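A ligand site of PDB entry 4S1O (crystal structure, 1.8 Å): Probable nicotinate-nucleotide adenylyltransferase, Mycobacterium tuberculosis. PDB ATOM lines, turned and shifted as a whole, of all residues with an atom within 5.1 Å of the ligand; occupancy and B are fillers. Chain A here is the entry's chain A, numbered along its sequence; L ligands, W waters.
Phe 14 touches the ligand (CZ to N3, 3.7 Å). Thr 85 touches the ligand (CG2 to O13, 3.2 Å). Tyr 86 touches the ligand. Phe 105 touches the ligand (CZ to O12, 3.6 Å). Thr 106 touches the ligand. N of Gly 108 touches C10 of the ligand, at 3.4 Å. Ala 111 touches the ligand. Trp 118 touches the ligand (NE1 to C19, 3.2 Å). CG2 of Val 133 touches C9 of the ligand, at 3.3 Å. Leu 165 touches the ligand (CD2 to C9, 3.9 Å). Ser 168 touches the ligand (CA to O15, 3.4 Å). Hydrophobic or aromatic side chains within 4 Å of the ligand: Met 10, Phe 14, His 18, His 21, Tyr 86, Phe 105, Ala 111, Trp 118, Val 133 and Leu 165. 21 residues have an atom within 4 Å of the ligand: Met 10, Gly 11, Gly 12, Thr 13, Phe 14, His 18, His 21, Thr 85, Tyr 86, Thr 87, Phe 105, Thr 106, Thr 107, Gly 108, Ala 111, Trp 118, Gln 119, Val 133, Leu 165, Ser 168 and Ser 169. Along chain A the residues within 4 Å of the ligand span positions 10 to 169.
A ring nitrogen (NE2) of His 18 lies within hydrogen-bond range of the backbone NH of Ser 169 (3.4 Å). A ring nitrogen (NE2) of His 18 lies close to the backbone carbonyl oxygen (O) of Ile 167. O of Gly 11 is in hydrogen-bond range of OG1 of Thr 107, 2.9 Å away. The backbone NH (N) of Gly 11 lies within hydrogen-bond range of the backbone carbonyl oxygen (O) of Thr 106 (2.9 Å). The backbone carbonyl oxygen (O) of Thr 107 lies within hydrogen-bond range of the backbone NH (N) of Val 133, 3.0 Å away. The side-chain hydroxyl (OG) of Ser 42 is in hydrogen-bond range of the side-chain hydroxyl (OG1) of Thr 13 (3.2 Å). The indole nitrogen (NE1) of Trp 118 lies within hydrogen-bond range of the side-chain hydroxyl (OG) of Ser 114, at 3.2 Å. The backbone carbonyl oxygen (O) of Gly 12 lies within hydrogen-bond range of the backbone NH (N) of Ser 42 (2.9 Å).
The backbone NH of Ser 169 is in hydrogen-bond range of an oxygen (O15) of the ligand, 2.8 Å away. O17 of the ligand is in hydrogen-bond range of OG of Ser 169, 2.5 Å away. NE2 of His 21 sits at hydrogen-bond distance from O16 of the ligand, 2.7 Å away. An oxygen (O15) of the ligand is in hydrogen-bond range of a ring nitrogen (NE2) of His 18. N of Thr 87 lies within hydrogen-bond range of O14 of the ligand (2.9 Å). OE1 of Gln 119 is in hydrogen-bond range of N7 of the ligand. The backbone carbonyl oxygen of Gly 11 lies within hydrogen-bond range of a nitrogen (N3) of the ligand, at 3.0 Å. A nitrogen (N2) of the ligand lies within hydrogen-bond range of the side-chain hydroxyl of Thr 107. N of Thr 13 sits at hydrogen-bond distance from O8 of the ligand (3.0 Å). The side-chain hydroxyl of Thr 13 sits at hydrogen-bond distance from an oxygen (O8) of the ligand (3.1 Å). The side-chain sulfur (SD) of Met 10 sits close to a nitrogen (N3) of the ligand. O12 of the ligand lies within hydrogen-bond range of N of Gly 12 (3.4 Å).
Water W6 lies within hydrogen-bond range of O16 of the ligand (2.6 Å), N of Phe 14 (3.1 Å) and N of Thr 13 (3.3 Å). Water W12 lies within hydrogen-bond range of O12 of the ligand (2.6 Å), OD2 of Asp 78 (2.8 Å) and O of Val 40 (2.8 Å). Water W13 lies within hydrogen-bond range of OG1 of Thr 170 and O17 of the ligand. Water W11 lies within hydrogen-bond range of the backbone carbonyl oxygen (O) of Ile 167 (2.8 Å), an oxygen (O15) of the ligand (2.8 Å) and the backbone carbonyl oxygen (O) of Leu 165 (3.3 Å). Water W2 lies within hydrogen-bond range of O of Gln 119 (2.8 Å), N of Lys 88 (2.9 Å), O14 of the ligand (2.9 Å) and N of Thr 87 (3.2 Å). Water W7 lies within hydrogen-bond range of OG1 of Thr 87 (3.0 Å) and O13 of the ligand (3.1 Å).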
ATOM      1  N   MET A  10      18.061  23.967  -9.529  1.00  0.00           N
ATOM      2  CA  MET A  10      17.569  23.920  -8.138  1.00  0.00           C
ATOM      3  C   MET A  10      16.628  22.741  -7.966  1.00  0.00           C
ATOM      4  O   MET A  10      15.454  22.808  -8.341  1.00  0.00           O
ATOM      5  CB  MET A  10      16.810  25.220  -7.791  1.00  0.00           C
ATOM      6  CG  MET A  10      17.718  26.304  -7.311  1.00  0.00           C
ATOM      7  SD  MET A  10      18.327  26.095  -5.638  1.00  0.00           S
ATOM      8  CE  MET A  10      16.894  26.682  -4.719  1.00  0.00           C
ATOM      9  N   GLY A  11      17.149  21.649  -7.411  1.00  0.00           N
ATOM     10  CA  GLY A  11      16.367  20.447  -7.169  1.00  0.00           C
ATOM     11  C   GLY A  11      15.832  20.473  -5.763  1.00  0.00           C
ATOM     12  O   GLY A  11      16.565  20.745  -4.838  1.00  0.00           O
ATOM     13  N   GLY A  12      14.547  20.175  -5.613  1.00  0.00           N
ATOM     14  CA  GLY A  12      13.950  20.045  -4.315  1.00  0.00           C
ATOM     15  C   GLY A  12      12.504  19.693  -4.418  1.00  0.00           C
ATOM     16  O   GLY A  12      11.940  19.643  -5.522  1.00  0.00           O
ATOM     17  N   THR A  13      11.894  19.432  -3.259  1.00  0.00           N
ATOM     18  CA  THR A  13      10.490  19.124  -3.216  1.00  0.00           C
ATOM     19  C   THR A  13       9.620  20.417  -3.315  1.00  0.00           C
ATOM     20  O   THR A  13       8.573  20.433  -3.996  1.00  0.00           O
ATOM     21  CB  THR A  13      10.184  18.269  -1.968  1.00  0.00           C
ATOM     22  OG1 THR A  13      10.828  16.998  -2.164  1.00  0.00           O
ATOM     23  CG2 THR A  13       8.718  18.011  -1.879  1.00  0.00           C
ATOM     24  N   PHE A  14      10.058  21.479  -2.633  1.00  0.00           N
ATOM     25  CA  PHE A  14       9.406  22.792  -2.700  1.00  0.00           C
ATOM     26  C   PHE A  14       7.931  22.722  -2.246  1.00  0.00           C
ATOM     27  O   PHE A  14       6.993  23.045  -2.990  1.00  0.00           O
ATOM     28  CB  PHE A  14       9.526  23.436  -4.088  1.00  0.00           C
ATOM     29  CG  PHE A  14      10.933  23.547  -4.591  1.00  0.00           C
ATOM     30  CD1 PHE A  14      11.935  24.114  -3.804  1.00  0.00           C
ATOM     31  CD2 PHE A  14      11.288  23.053  -5.831  1.00  0.00           C
ATOM     32  CE1 PHE A  14      13.238  24.205  -4.262  1.00  0.00           C
ATOM     33  CE2 PHE A  14      12.599  23.124  -6.295  1.00  0.00           C
ATOM     34  CZ  PHE A  14      13.576  23.674  -5.506  1.00  0.00           C
ATOM     35  N   HIS A  18       9.982  28.845  -0.593  1.00  0.00           N
ATOM     36  CA  HIS A  18      10.027  29.988   0.313  1.00  0.00           C
ATOM     37  C   HIS A  18      11.217  30.869  -0.014  1.00  0.00           C
ATOM     38  O   HIS A  18      12.032  30.539  -0.879  1.00  0.00           O
ATOM     39  CB  HIS A  18      10.040  29.508   1.772  1.00  0.00           C
ATOM     40  CG  HIS A  18      11.100  28.512   2.059  1.00  0.00           C
ATOM     41  ND1 HIS A  18      12.436  28.835   2.016  1.00  0.00           N
ATOM     42  CD2 HIS A  18      11.046  27.209   2.407  1.00  0.00           C
ATOM     43  CE1 HIS A  18      13.152  27.779   2.328  1.00  0.00           C
ATOM     44  NE2 HIS A  18      12.340  26.779   2.564  1.00  0.00           N
ATOM     45  N   HIS A  21      14.835  29.408  -0.368  1.00  0.00           N
ATOM     46  CA  HIS A  21      15.167  28.767  -1.642  1.00  0.00           C
ATOM     47  C   HIS A  21      15.564  29.845  -2.671  1.00  0.00           C
ATOM     48  O   HIS A  21      16.542  29.693  -3.418  1.00  0.00           O
ATOM     49  CB  HIS A  21      13.979  27.991  -2.221  1.00  0.00           C
ATOM     50  CG  HIS A  21      13.534  26.835  -1.385  1.00  0.00           C
ATOM     51  ND1 HIS A  21      12.252  26.715  -0.917  1.00  0.00           N
ATOM     52  CD2 HIS A  21      14.175  25.737  -0.946  1.00  0.00           C
ATOM     53  CE1 HIS A  21      12.114  25.595  -0.248  1.00  0.00           C
ATOM     54  NE2 HIS A  21      13.276  24.975  -0.241  1.00  0.00           N
ATOM     55  N   ALA A  24      18.834  31.480  -1.877  1.00  0.00           N
ATOM     56  CA  ALA A  24      19.888  30.495  -2.176  1.00  0.00           C
ATOM     57  C   ALA A  24      20.177  30.446  -3.680  1.00  0.00           C
ATOM     58  O   ALA A  24      21.332  30.539  -4.078  1.00  0.00           O
ATOM     59  CB  ALA A  24      19.517  29.138  -1.650  1.00  0.00           C
ATOM     60  N   VAL A  40      13.532  22.673 -10.423  1.00  0.00           N
ATOM     61  CA  VAL A  40      12.986  21.380 -10.828  1.00  0.00           C
ATOM     62  C   VAL A  40      12.334  20.734  -9.618  1.00  0.00           C
ATOM     63  O   VAL A  40      13.011  20.043  -8.804  1.00  0.00           O
ATOM     64  CB  VAL A  40      14.070  20.460 -11.438  1.00  0.00           C
ATOM     65  CG1 VAL A  40      13.438  19.209 -12.002  1.00  0.00           C
ATOM     66  CG2 VAL A  40      14.838  21.220 -12.520  1.00  0.00           C
ATOM     67  N   SER A  42      10.639  18.028  -7.487  1.00  0.00           N
ATOM     68  CA  SER A  42      10.833  16.589  -7.672  1.00  0.00           C
ATOM     69  C   SER A  42       9.509  15.885  -7.875  1.00  0.00           C
ATOM     70  O   SER A  42       8.442  16.434  -7.521  1.00  0.00           O
ATOM     71  CB  SER A  42      11.595  16.000  -6.492  1.00  0.00           C
ATOM     72  OG  SER A  42      10.921  16.287  -5.303  1.00  0.00           O
ATOM     73  N   ASP A  78      11.074  16.319 -13.845  1.00  0.00           N
ATOM     74  CA  ASP A  78      10.945  15.297 -12.792  1.00  0.00           C
ATOM     75  C   ASP A  78       9.495  14.938 -12.568  1.00  0.00           C
ATOM     76  O   ASP A  78       9.154  13.745 -12.377  1.00  0.00           O
ATOM     77  CB  ASP A  78      11.567  15.749 -11.477  1.00  0.00           C
ATOM     78  CG  ASP A  78      13.086  15.763 -11.522  1.00  0.00           C
ATOM     79  OD1 ASP A  78      13.701  15.194 -12.477  1.00  0.00           O
ATOM     80  OD2 ASP A  78      13.674  16.327 -10.566  1.00  0.00           O
ATOM     81  N   THR A  85      11.903  10.398  -8.425  1.00  0.00           N
ATOM     82  CA  THR A  85      12.958  11.192  -9.039  1.00  0.00           C
ATOM     83  C   THR A  85      14.349  10.750  -8.625  1.00  0.00           C
ATOM     84  O   THR A  85      14.634  10.614  -7.453  1.00  0.00           O
ATOM     85  CB  THR A  85      12.743  12.662  -8.674  1.00  0.00           C
ATOM     86  OG1 THR A  85      11.537  13.070  -9.322  1.00  0.00           O
ATOM     87  CG2 THR A  85      13.918  13.553  -9.121  1.00  0.00           C
ATOM     88  N   TYR A  86      15.207  10.525  -9.618  1.00  0.00           N
ATOM     89  CA  TYR A  86      16.608  10.227  -9.421  1.00  0.00           C
ATOM     90  C   TYR A  86      17.349  11.304 -10.202  1.00  0.00           C
ATOM     91  O   TYR A  86      17.057  11.574 -11.356  1.00  0.00           O
ATOM     92  CB  TYR A  86      16.976   8.827  -9.938  1.00  0.00           C
ATOM     93  CG  TYR A  86      15.979   7.731  -9.545  1.00  0.00           C
ATOM     94  CD1 TYR A  86      15.535   7.621  -8.242  1.00  0.00           C
ATOM     95  CD2 TYR A  86      15.489   6.836 -10.476  1.00  0.00           C
ATOM     96  CE1 TYR A  86      14.613   6.632  -7.870  1.00  0.00           C
ATOM     97  CE2 TYR A  86      14.577   5.839 -10.129  1.00  0.00           C
ATOM     98  CZ  TYR A  86      14.139   5.762  -8.810  1.00  0.00           C
ATOM     99  OH  TYR A  86      13.241   4.793  -8.419  1.00  0.00           O
ATOM    100  N   THR A  87      18.333  11.898  -9.574  1.00  0.00           N
ATOM    101  CA  THR A  87      19.026  13.039 -10.173  1.00  0.00           C
ATOM    102  C   THR A  87      19.800  12.724 -11.456  1.00  0.00           C
ATOM    103  O   THR A  87      19.942  13.597 -12.322  1.00  0.00           O
ATOM    104  CB  THR A  87      19.914  13.674  -9.113  1.00  0.00           C
ATOM    105  OG1 THR A  87      19.071  14.078  -8.036  1.00  0.00           O
ATOM    106  CG2 THR A  87      20.676  14.914  -9.668  1.00  0.00           C
ATOM    107  N   LYS A  88      20.297  11.493 -11.595  1.00  0.00           N
ATOM    108  CA  LYS A  88      20.881  11.086 -12.868  1.00  0.00           C
ATOM    109  C   LYS A  88      19.936  11.297 -14.032  1.00  0.00           C
ATOM    110  O   LYS A  88      20.383  11.711 -15.098  1.00  0.00           O
ATOM    111  CB  LYS A  88      21.440   9.642 -12.844  1.00  0.00           C
ATOM    112  CG  LYS A  88      20.387   8.549 -12.784  1.00  0.00           C
ATOM    113  CD  LYS A  88      20.974   7.146 -12.801  1.00  0.00           C
ATOM    114  CE  LYS A  88      19.862   6.127 -12.637  1.00  0.00           C
ATOM    115  NZ  LYS A  88      18.875   6.180 -13.727  1.00  0.00           N
ATOM    116  N   PHE A 105      24.122  21.652 -10.151  1.00  0.00           N
ATOM    117  CA  PHE A 105      23.009  21.083  -9.426  1.00  0.00           C
ATOM    118  C   PHE A 105      23.089  21.554  -7.998  1.00  0.00           C
ATOM    119  O   PHE A 105      24.095  21.317  -7.317  1.00  0.00           O
ATOM    120  CB  PHE A 105      23.018  19.574  -9.471  1.00  0.00           C
ATOM    121  CG  PHE A 105      21.815  18.962  -8.815  1.00  0.00           C
ATOM    122  CD1 PHE A 105      20.608  18.912  -9.499  1.00  0.00           C
ATOM    123  CD2 PHE A 105      21.868  18.486  -7.523  1.00  0.00           C
ATOM    124  CE1 PHE A 105      19.482  18.378  -8.900  1.00  0.00           C
ATOM    125  CE2 PHE A 105      20.736  17.944  -6.924  1.00  0.00           C
ATOM    126  CZ  PHE A 105      19.558  17.884  -7.618  1.00  0.00           C
ATOM    127  N   THR A 106      22.015  22.199  -7.550  1.00  0.00           N
ATOM    128  CA  THR A 106      21.962  22.837  -6.244  1.00  0.00           C
ATOM    129  C   THR A 106      20.796  22.299  -5.446  1.00  0.00           C
ATOM    130  O   THR A 106      19.644  22.245  -5.956  1.00  0.00           O
ATOM    131  CB  THR A 106      21.801  24.375  -6.395  1.00  0.00           C
ATOM    132  OG1 THR A 106      22.805  24.875  -7.284  1.00  0.00           O
ATOM    133  CG2 THR A 106      21.930  25.061  -5.064  1.00  0.00           C
ATOM    134  N   THR A 107      21.092  21.835  -4.236  1.00  0.00           N
ATOM    135  CA  THR A 107      20.068  21.453  -3.298  1.00  0.00           C
ATOM    136  C   THR A 107      20.593  21.549  -1.859  1.00  0.00           C
ATOM    137  O   THR A 107      21.703  22.027  -1.613  1.00  0.00           O
ATOM    138  CB  THR A 107      19.509  20.057  -3.635  1.00  0.00           C
ATOM    139  OG1 THR A 107      18.392  19.798  -2.796  1.00  0.00           O
ATOM    140  CG2 THR A 107      20.556  18.931  -3.392  1.00  0.00           C
ATOM    141  N   GLY A 108      19.775  21.144  -0.895  1.00  0.00           N
ATOM    142  CA  GLY A 108      20.163  21.208   0.500  1.00  0.00           C
ATOM    143  C   GLY A 108      21.388  20.349   0.760  1.00  0.00           C
ATOM    144  O   GLY A 108      21.490  19.234   0.252  1.00  0.00           O
ATOM    145  N   ALA A 109      22.322  20.856   1.562  1.00  0.00           N
ATOM    146  CA  ALA A 109      23.520  20.096   1.922  1.00  0.00           C
ATOM    147  C   ALA A 109      23.152  18.776   2.611  1.00  0.00           C
ATOM    148  O   ALA A 109      23.804  17.765   2.360  1.00  0.00           O
ATOM    149  CB  ALA A 109      24.443  20.917   2.810  1.00  0.00           C
ATOM    150  N   ASP A 110      22.090  18.791   3.416  1.00  0.00           N
ATOM    151  CA  ASP A 110      21.621  17.576   4.048  1.00  0.00           C
ATOM    152  C   ASP A 110      21.092  16.545   3.058  1.00  0.00           C
ATOM    153  O   ASP A 110      21.232  15.369   3.307  1.00  0.00           O
ATOM    154  CB  ASP A 110      20.572  17.850   5.132  1.00  0.00           C
ATOM    155  CG  ASP A 110      20.504  16.717   6.158  1.00  0.00           C
ATOM    156  OD1 ASP A 110      21.565  16.385   6.763  1.00  0.00           O
ATOM    157  OD2 ASP A 110      19.412  16.127   6.327  1.00  0.00           O
ATOM    158  N   ALA A 111      20.482  16.964   1.953  1.00  0.00           N
ATOM    159  CA  ALA A 111      20.123  16.028   0.864  1.00  0.00           C
ATOM    160  C   ALA A 111      21.364  15.390   0.227  1.00  0.00           C
ATOM    161  O   ALA A 111      21.394  14.206  -0.065  1.00  0.00           O
ATOM    162  CB  ALA A 111      19.348  16.755  -0.222  1.00  0.00           C
ATOM    163  N   SER A 114      23.705  12.199   1.412  1.00  0.00           N
ATOM    164  CA  SER A 114      23.410  10.812   1.017  1.00  0.00           C
ATOM    165  C   SER A 114      23.784  10.518  -0.431  1.00  0.00           C
ATOM    166  O   SER A 114      23.389   9.463  -0.955  1.00  0.00           O
ATOM    167  CB  SER A 114      21.934  10.487   1.275  1.00  0.00           C
ATOM    168  OG  SER A 114      21.053  11.286   0.472  1.00  0.00           O
ATOM    169  N   TRP A 118      22.930   7.619  -4.173  1.00  0.00           N
ATOM    170  CA  TRP A 118      22.165   7.943  -5.372  1.00  0.00           C
ATOM    171  C   TRP A 118      22.696   7.095  -6.549  1.00  0.00           C
ATOM    172  O   TRP A 118      23.895   6.839  -6.628  1.00  0.00           O
ATOM    173  CB  TRP A 118      22.272   9.420  -5.731  1.00  0.00           C
ATOM    174  CG  TRP A 118      21.775  10.380  -4.688  1.00  0.00           C
ATOM    175  CD1 TRP A 118      21.458  10.120  -3.374  1.00  0.00           C
ATOM    176  CD2 TRP A 118      21.619  11.798  -4.854  1.00  0.00           C
ATOM    177  NE1 TRP A 118      21.104  11.269  -2.731  1.00  0.00           N
ATOM    178  CE2 TRP A 118      21.197  12.319  -3.601  1.00  0.00           C
ATOM    179  CE3 TRP A 118      21.793  12.683  -5.926  1.00  0.00           C
ATOM    180  CZ2 TRP A 118      20.913  13.664  -3.422  1.00  0.00           C
ATOM    181  CZ3 TRP A 118      21.540  14.015  -5.746  1.00  0.00           C
ATOM    182  CH2 TRP A 118      21.098  14.501  -4.505  1.00  0.00           C
ATOM    183  N   GLN A 119      21.814   6.725  -7.454  1.00  0.00           N
ATOM    184  CA  GLN A 119      22.167   5.953  -8.623  1.00  0.00           C
ATOM    185  C   GLN A 119      23.071   6.787  -9.515  1.00  0.00           C
ATOM    186  O   GLN A 119      22.870   8.012  -9.654  1.00  0.00           O
ATOM    187  CB  GLN A 119      20.944   5.560  -9.433  1.00  0.00           C
ATOM    188  CG  GLN A 119      19.922   4.754  -8.683  1.00  0.00           C
ATOM    189  CD  GLN A 119      18.786   5.613  -8.146  1.00  0.00           C
ATOM    190  OE1 GLN A 119      19.012   6.675  -7.555  1.00  0.00           O
ATOM    191  NE2 GLN A 119      17.581   5.147  -8.323  1.00  0.00           N
ATOM    192  N   VAL A 133      23.681  23.816  -0.347  1.00  0.00           N
ATOM    193  CA  VAL A 133      23.394  25.041   0.409  1.00  0.00           C
ATOM    194  C   VAL A 133      22.803  24.652   1.759  1.00  0.00           C
ATOM    195  O   VAL A 133      21.982  23.721   1.843  1.00  0.00           O
ATOM    196  CB  VAL A 133      22.447  26.007  -0.354  1.00  0.00           C
ATOM    197  CG1 VAL A 133      23.140  26.558  -1.573  1.00  0.00           C
ATOM    198  CG2 VAL A 133      21.153  25.329  -0.760  1.00  0.00           C
ATOM    199  N   LEU A 165      18.323  30.388   4.752  1.00  0.00           N
ATOM    200  CA  LEU A 165      17.882  28.994   4.826  1.00  0.00           C
ATOM    201  C   LEU A 165      17.589  28.524   6.240  1.00  0.00           C
ATOM    202  O   LEU A 165      17.207  27.376   6.441  1.00  0.00           O
ATOM    203  CB  LEU A 165      18.869  28.021   4.147  1.00  0.00           C
ATOM    204  CG  LEU A 165      18.922  28.143   2.622  1.00  0.00           C
ATOM    205  CD1 LEU A 165      20.028  27.206   2.129  1.00  0.00           C
ATOM    206  CD2 LEU A 165      17.596  27.743   1.995  1.00  0.00           C
ATOM    207  N   ILE A 167      14.927  29.658   7.197  1.00  0.00           N
ATOM    208  CA  ILE A 167      13.509  29.471   6.783  1.00  0.00           C
ATOM    209  C   ILE A 167      13.378  28.094   6.148  1.00  0.00           C
ATOM    210  O   ILE A 167      14.163  27.799   5.244  1.00  0.00           O
ATOM    211  CB  ILE A 167      13.052  30.521   5.751  1.00  0.00           C
ATOM    212  CG1 ILE A 167      13.167  31.937   6.303  1.00  0.00           C
ATOM    213  CG2 ILE A 167      11.600  30.259   5.299  1.00  0.00           C
ATOM    214  CD1 ILE A 167      13.058  33.056   5.267  1.00  0.00           C
ATOM    215  N   SER A 168      12.449  27.276   6.630  1.00  0.00           N
ATOM    216  CA  SER A 168      12.349  25.875   6.182  1.00  0.00           C
ATOM    217  C   SER A 168      10.915  25.612   5.746  1.00  0.00           C
ATOM    218  O   SER A 168       9.956  26.218   6.251  1.00  0.00           O
ATOM    219  CB  SER A 168      12.809  24.901   7.270  1.00  0.00           C
ATOM    220  OG  SER A 168      11.872  24.832   8.310  1.00  0.00           O
ATOM    221  N   SER A 169      10.754  24.700   4.800  1.00  0.00           N
ATOM    222  CA  SER A 169       9.423  24.342   4.340  1.00  0.00           C
ATOM    223  C   SER A 169       8.619  23.624   5.450  1.00  0.00           C
ATOM    224  O   SER A 169       7.422  23.815   5.557  1.00  0.00           O
ATOM    225  CB  SER A 169       9.512  23.498   3.058  1.00  0.00           C
ATOM    226  OG  SER A 169       9.905  22.148   3.281  1.00  0.00           O
ATOM    227  N   THR A 170       9.290  22.823   6.265  1.00  0.00           N
ATOM    228  CA  THR A 170       8.636  22.178   7.403  1.00  0.00           C
ATOM    229  C   THR A 170       8.016  23.196   8.363  1.00  0.00           C
ATOM    230  O   THR A 170       6.877  23.026   8.815  1.00  0.00           O
ATOM    231  CB  THR A 170       9.650  21.337   8.152  1.00  0.00           C
ATOM    232  OG1 THR A 170      10.157  20.345   7.258  1.00  0.00           O
ATOM    233  CG2 THR A 170       9.016  20.637   9.379  1.00  0.00           C
HETATM  234  P1  LIG L   1      14.498  17.071   1.407  1.00  0.00           P
HETATM  235  O1  LIG L   1      14.919  15.818   2.157  1.00  0.00           O
HETATM  236  O2  LIG L   1      13.093  17.512   1.218  1.00  0.00           O
HETATM  237  O3  LIG L   1      15.365  18.278   2.006  1.00  0.00           O
HETATM  238  C1  LIG L   1      16.484  18.105   2.870  1.00  0.00           C
HETATM  239  C2  LIG L   1      16.974  19.479   3.211  1.00  0.00           C
HETATM  240  O4  LIG L   1      17.313  20.142   1.990  1.00  0.00           O
HETATM  241  C3  LIG L   1      15.902  20.339   3.868  1.00  0.00           C
HETATM  242  O5  LIG L   1      16.534  21.149   4.851  1.00  0.00           O
HETATM  243  C4  LIG L   1      15.353  21.193   2.727  1.00  0.00           C
HETATM  244  O6  LIG L   1      14.838  22.441   3.116  1.00  0.00           O
HETATM  245  C5  LIG L   1      16.617  21.401   1.923  1.00  0.00           C
HETATM  246  N1  LIG L   1      16.478  21.663   0.475  1.00  0.00           N
HETATM  247  C6  LIG L   1      15.965  20.811  -0.431  1.00  0.00           C
HETATM  248  N2  LIG L   1      16.055  21.315  -1.659  1.00  0.00           N
HETATM  249  C7  LIG L   1      16.628  22.532  -1.529  1.00  0.00           C
HETATM  250  C8  LIG L   1      17.055  23.612  -2.427  1.00  0.00           C
HETATM  251  N3  LIG L   1      16.840  23.477  -3.754  1.00  0.00           N
HETATM  252  N4  LIG L   1      17.668  24.700  -1.890  1.00  0.00           N
HETATM  253  C9  LIG L   1      17.876  24.841  -0.560  1.00  0.00           C
HETATM  254  N5  LIG L   1      17.513  23.888   0.315  1.00  0.00           N
HETATM  255  C10 LIG L   1      16.927  22.729  -0.117  1.00  0.00           C
HETATM  256  O7  LIG L   1      15.252  17.012   0.011  1.00  0.00           O
HETATM  257  P2  LIG L   1      14.562  16.513  -1.317  1.00  0.00           P
HETATM  258  O8  LIG L   1      13.760  17.777  -1.523  1.00  0.00           O
HETATM  259  O9  LIG L   1      14.150  15.070  -1.081  1.00  0.00           O
HETATM  260  O10 LIG L   1      15.746  16.272  -2.398  1.00  0.00           O
HETATM  261  C11 LIG L   1      16.581  17.304  -2.802  1.00  0.00           C
HETATM  262  C12 LIG L   1      17.062  17.015  -4.225  1.00  0.00           C
HETATM  263  O11 LIG L   1      17.947  15.874  -4.184  1.00  0.00           O
HETATM  264  C13 LIG L   1      15.923  16.681  -5.172  1.00  0.00           C
HETATM  265  O12 LIG L   1      16.193  17.322  -6.421  1.00  0.00           O
HETATM  266  C14 LIG L   1      16.018  15.167  -5.293  1.00  0.00           C
HETATM  267  O13 LIG L   1      15.561  14.638  -6.550  1.00  0.00           O
HETATM  268  C15 LIG L   1      17.510  14.899  -5.092  1.00  0.00           C
HETATM  269  N6  LIG L   1      17.700  13.534  -4.557  1.00  0.00           N
HETATM  270  C16 LIG L   1      18.021  12.561  -5.420  1.00  0.00           C
HETATM  271  C17 LIG L   1      18.228  11.232  -5.008  1.00  0.00           C
HETATM  272  C18 LIG L   1      18.575  10.199  -6.047  1.00  0.00           C
HETATM  273  O14 LIG L   1      19.050  10.567  -7.119  1.00  0.00           O
HETATM  274  N7  LIG L   1      18.332   8.904  -5.816  1.00  0.00           N
HETATM  275  C19 LIG L   1      18.016  10.927  -3.645  1.00  0.00           C
HETATM  276  C20 LIG L   1      17.659  11.967  -2.770  1.00  0.00           C
HETATM  277  C21 LIG L   1      17.498  13.272  -3.251  1.00  0.00           C
HETATM  278  P3  LIG L   1      13.335  22.817   2.718  1.00  0.00           P
HETATM  279  O15 LIG L   1      13.146  24.206   3.334  1.00  0.00           O
HETATM  280  O16 LIG L   1      13.356  22.750   1.217  1.00  0.00           O
HETATM  281  O17 LIG L   1      12.417  21.815   3.350  1.00  0.00           O
HETATM  282  O   HOH W   1      10.582  16.344   1.138  1.00  0.00           O
HETATM  283  O   HOH W   2      20.548   9.585  -9.426  1.00  0.00           O
HETATM  284  O   HOH W   3      12.363  19.162   3.424  1.00  0.00           O
HETATM  285  O   HOH W   4      14.485  21.600   7.450  1.00  0.00           O
HETATM  286  O   HOH W   5      15.887  23.272   6.097  1.00  0.00           O
HETATM  287  O   HOH W   6      12.187  21.060  -0.355  1.00  0.00           O
HETATM  288  O   HOH W   7      16.861  15.742  -9.133  1.00  0.00           O
HETATM  289  O   HOH W   8      17.862  24.465   2.998  1.00  0.00           O
HETATM  290  O   HOH W   9      17.661  14.867   3.150  1.00  0.00           O
HETATM  291  O   HOH W  10      18.530  12.989   0.389  1.00  0.00           O
HETATM  292  O   HOH W  11      15.481  25.483   4.301  1.00  0.00           O
HETATM  293  O   HOH W  12      14.236  17.586  -8.152  1.00  0.00           O
HETATM  294  O   HOH W  13      12.046  21.660   6.014  1.00  0.00           O
HETATM  295  O   HOH W  14      14.586  12.462  -5.565  1.00  0.00           O
HETATM  296  O   HOH W  15      16.244   8.108  -3.841  1.00  0.00           O
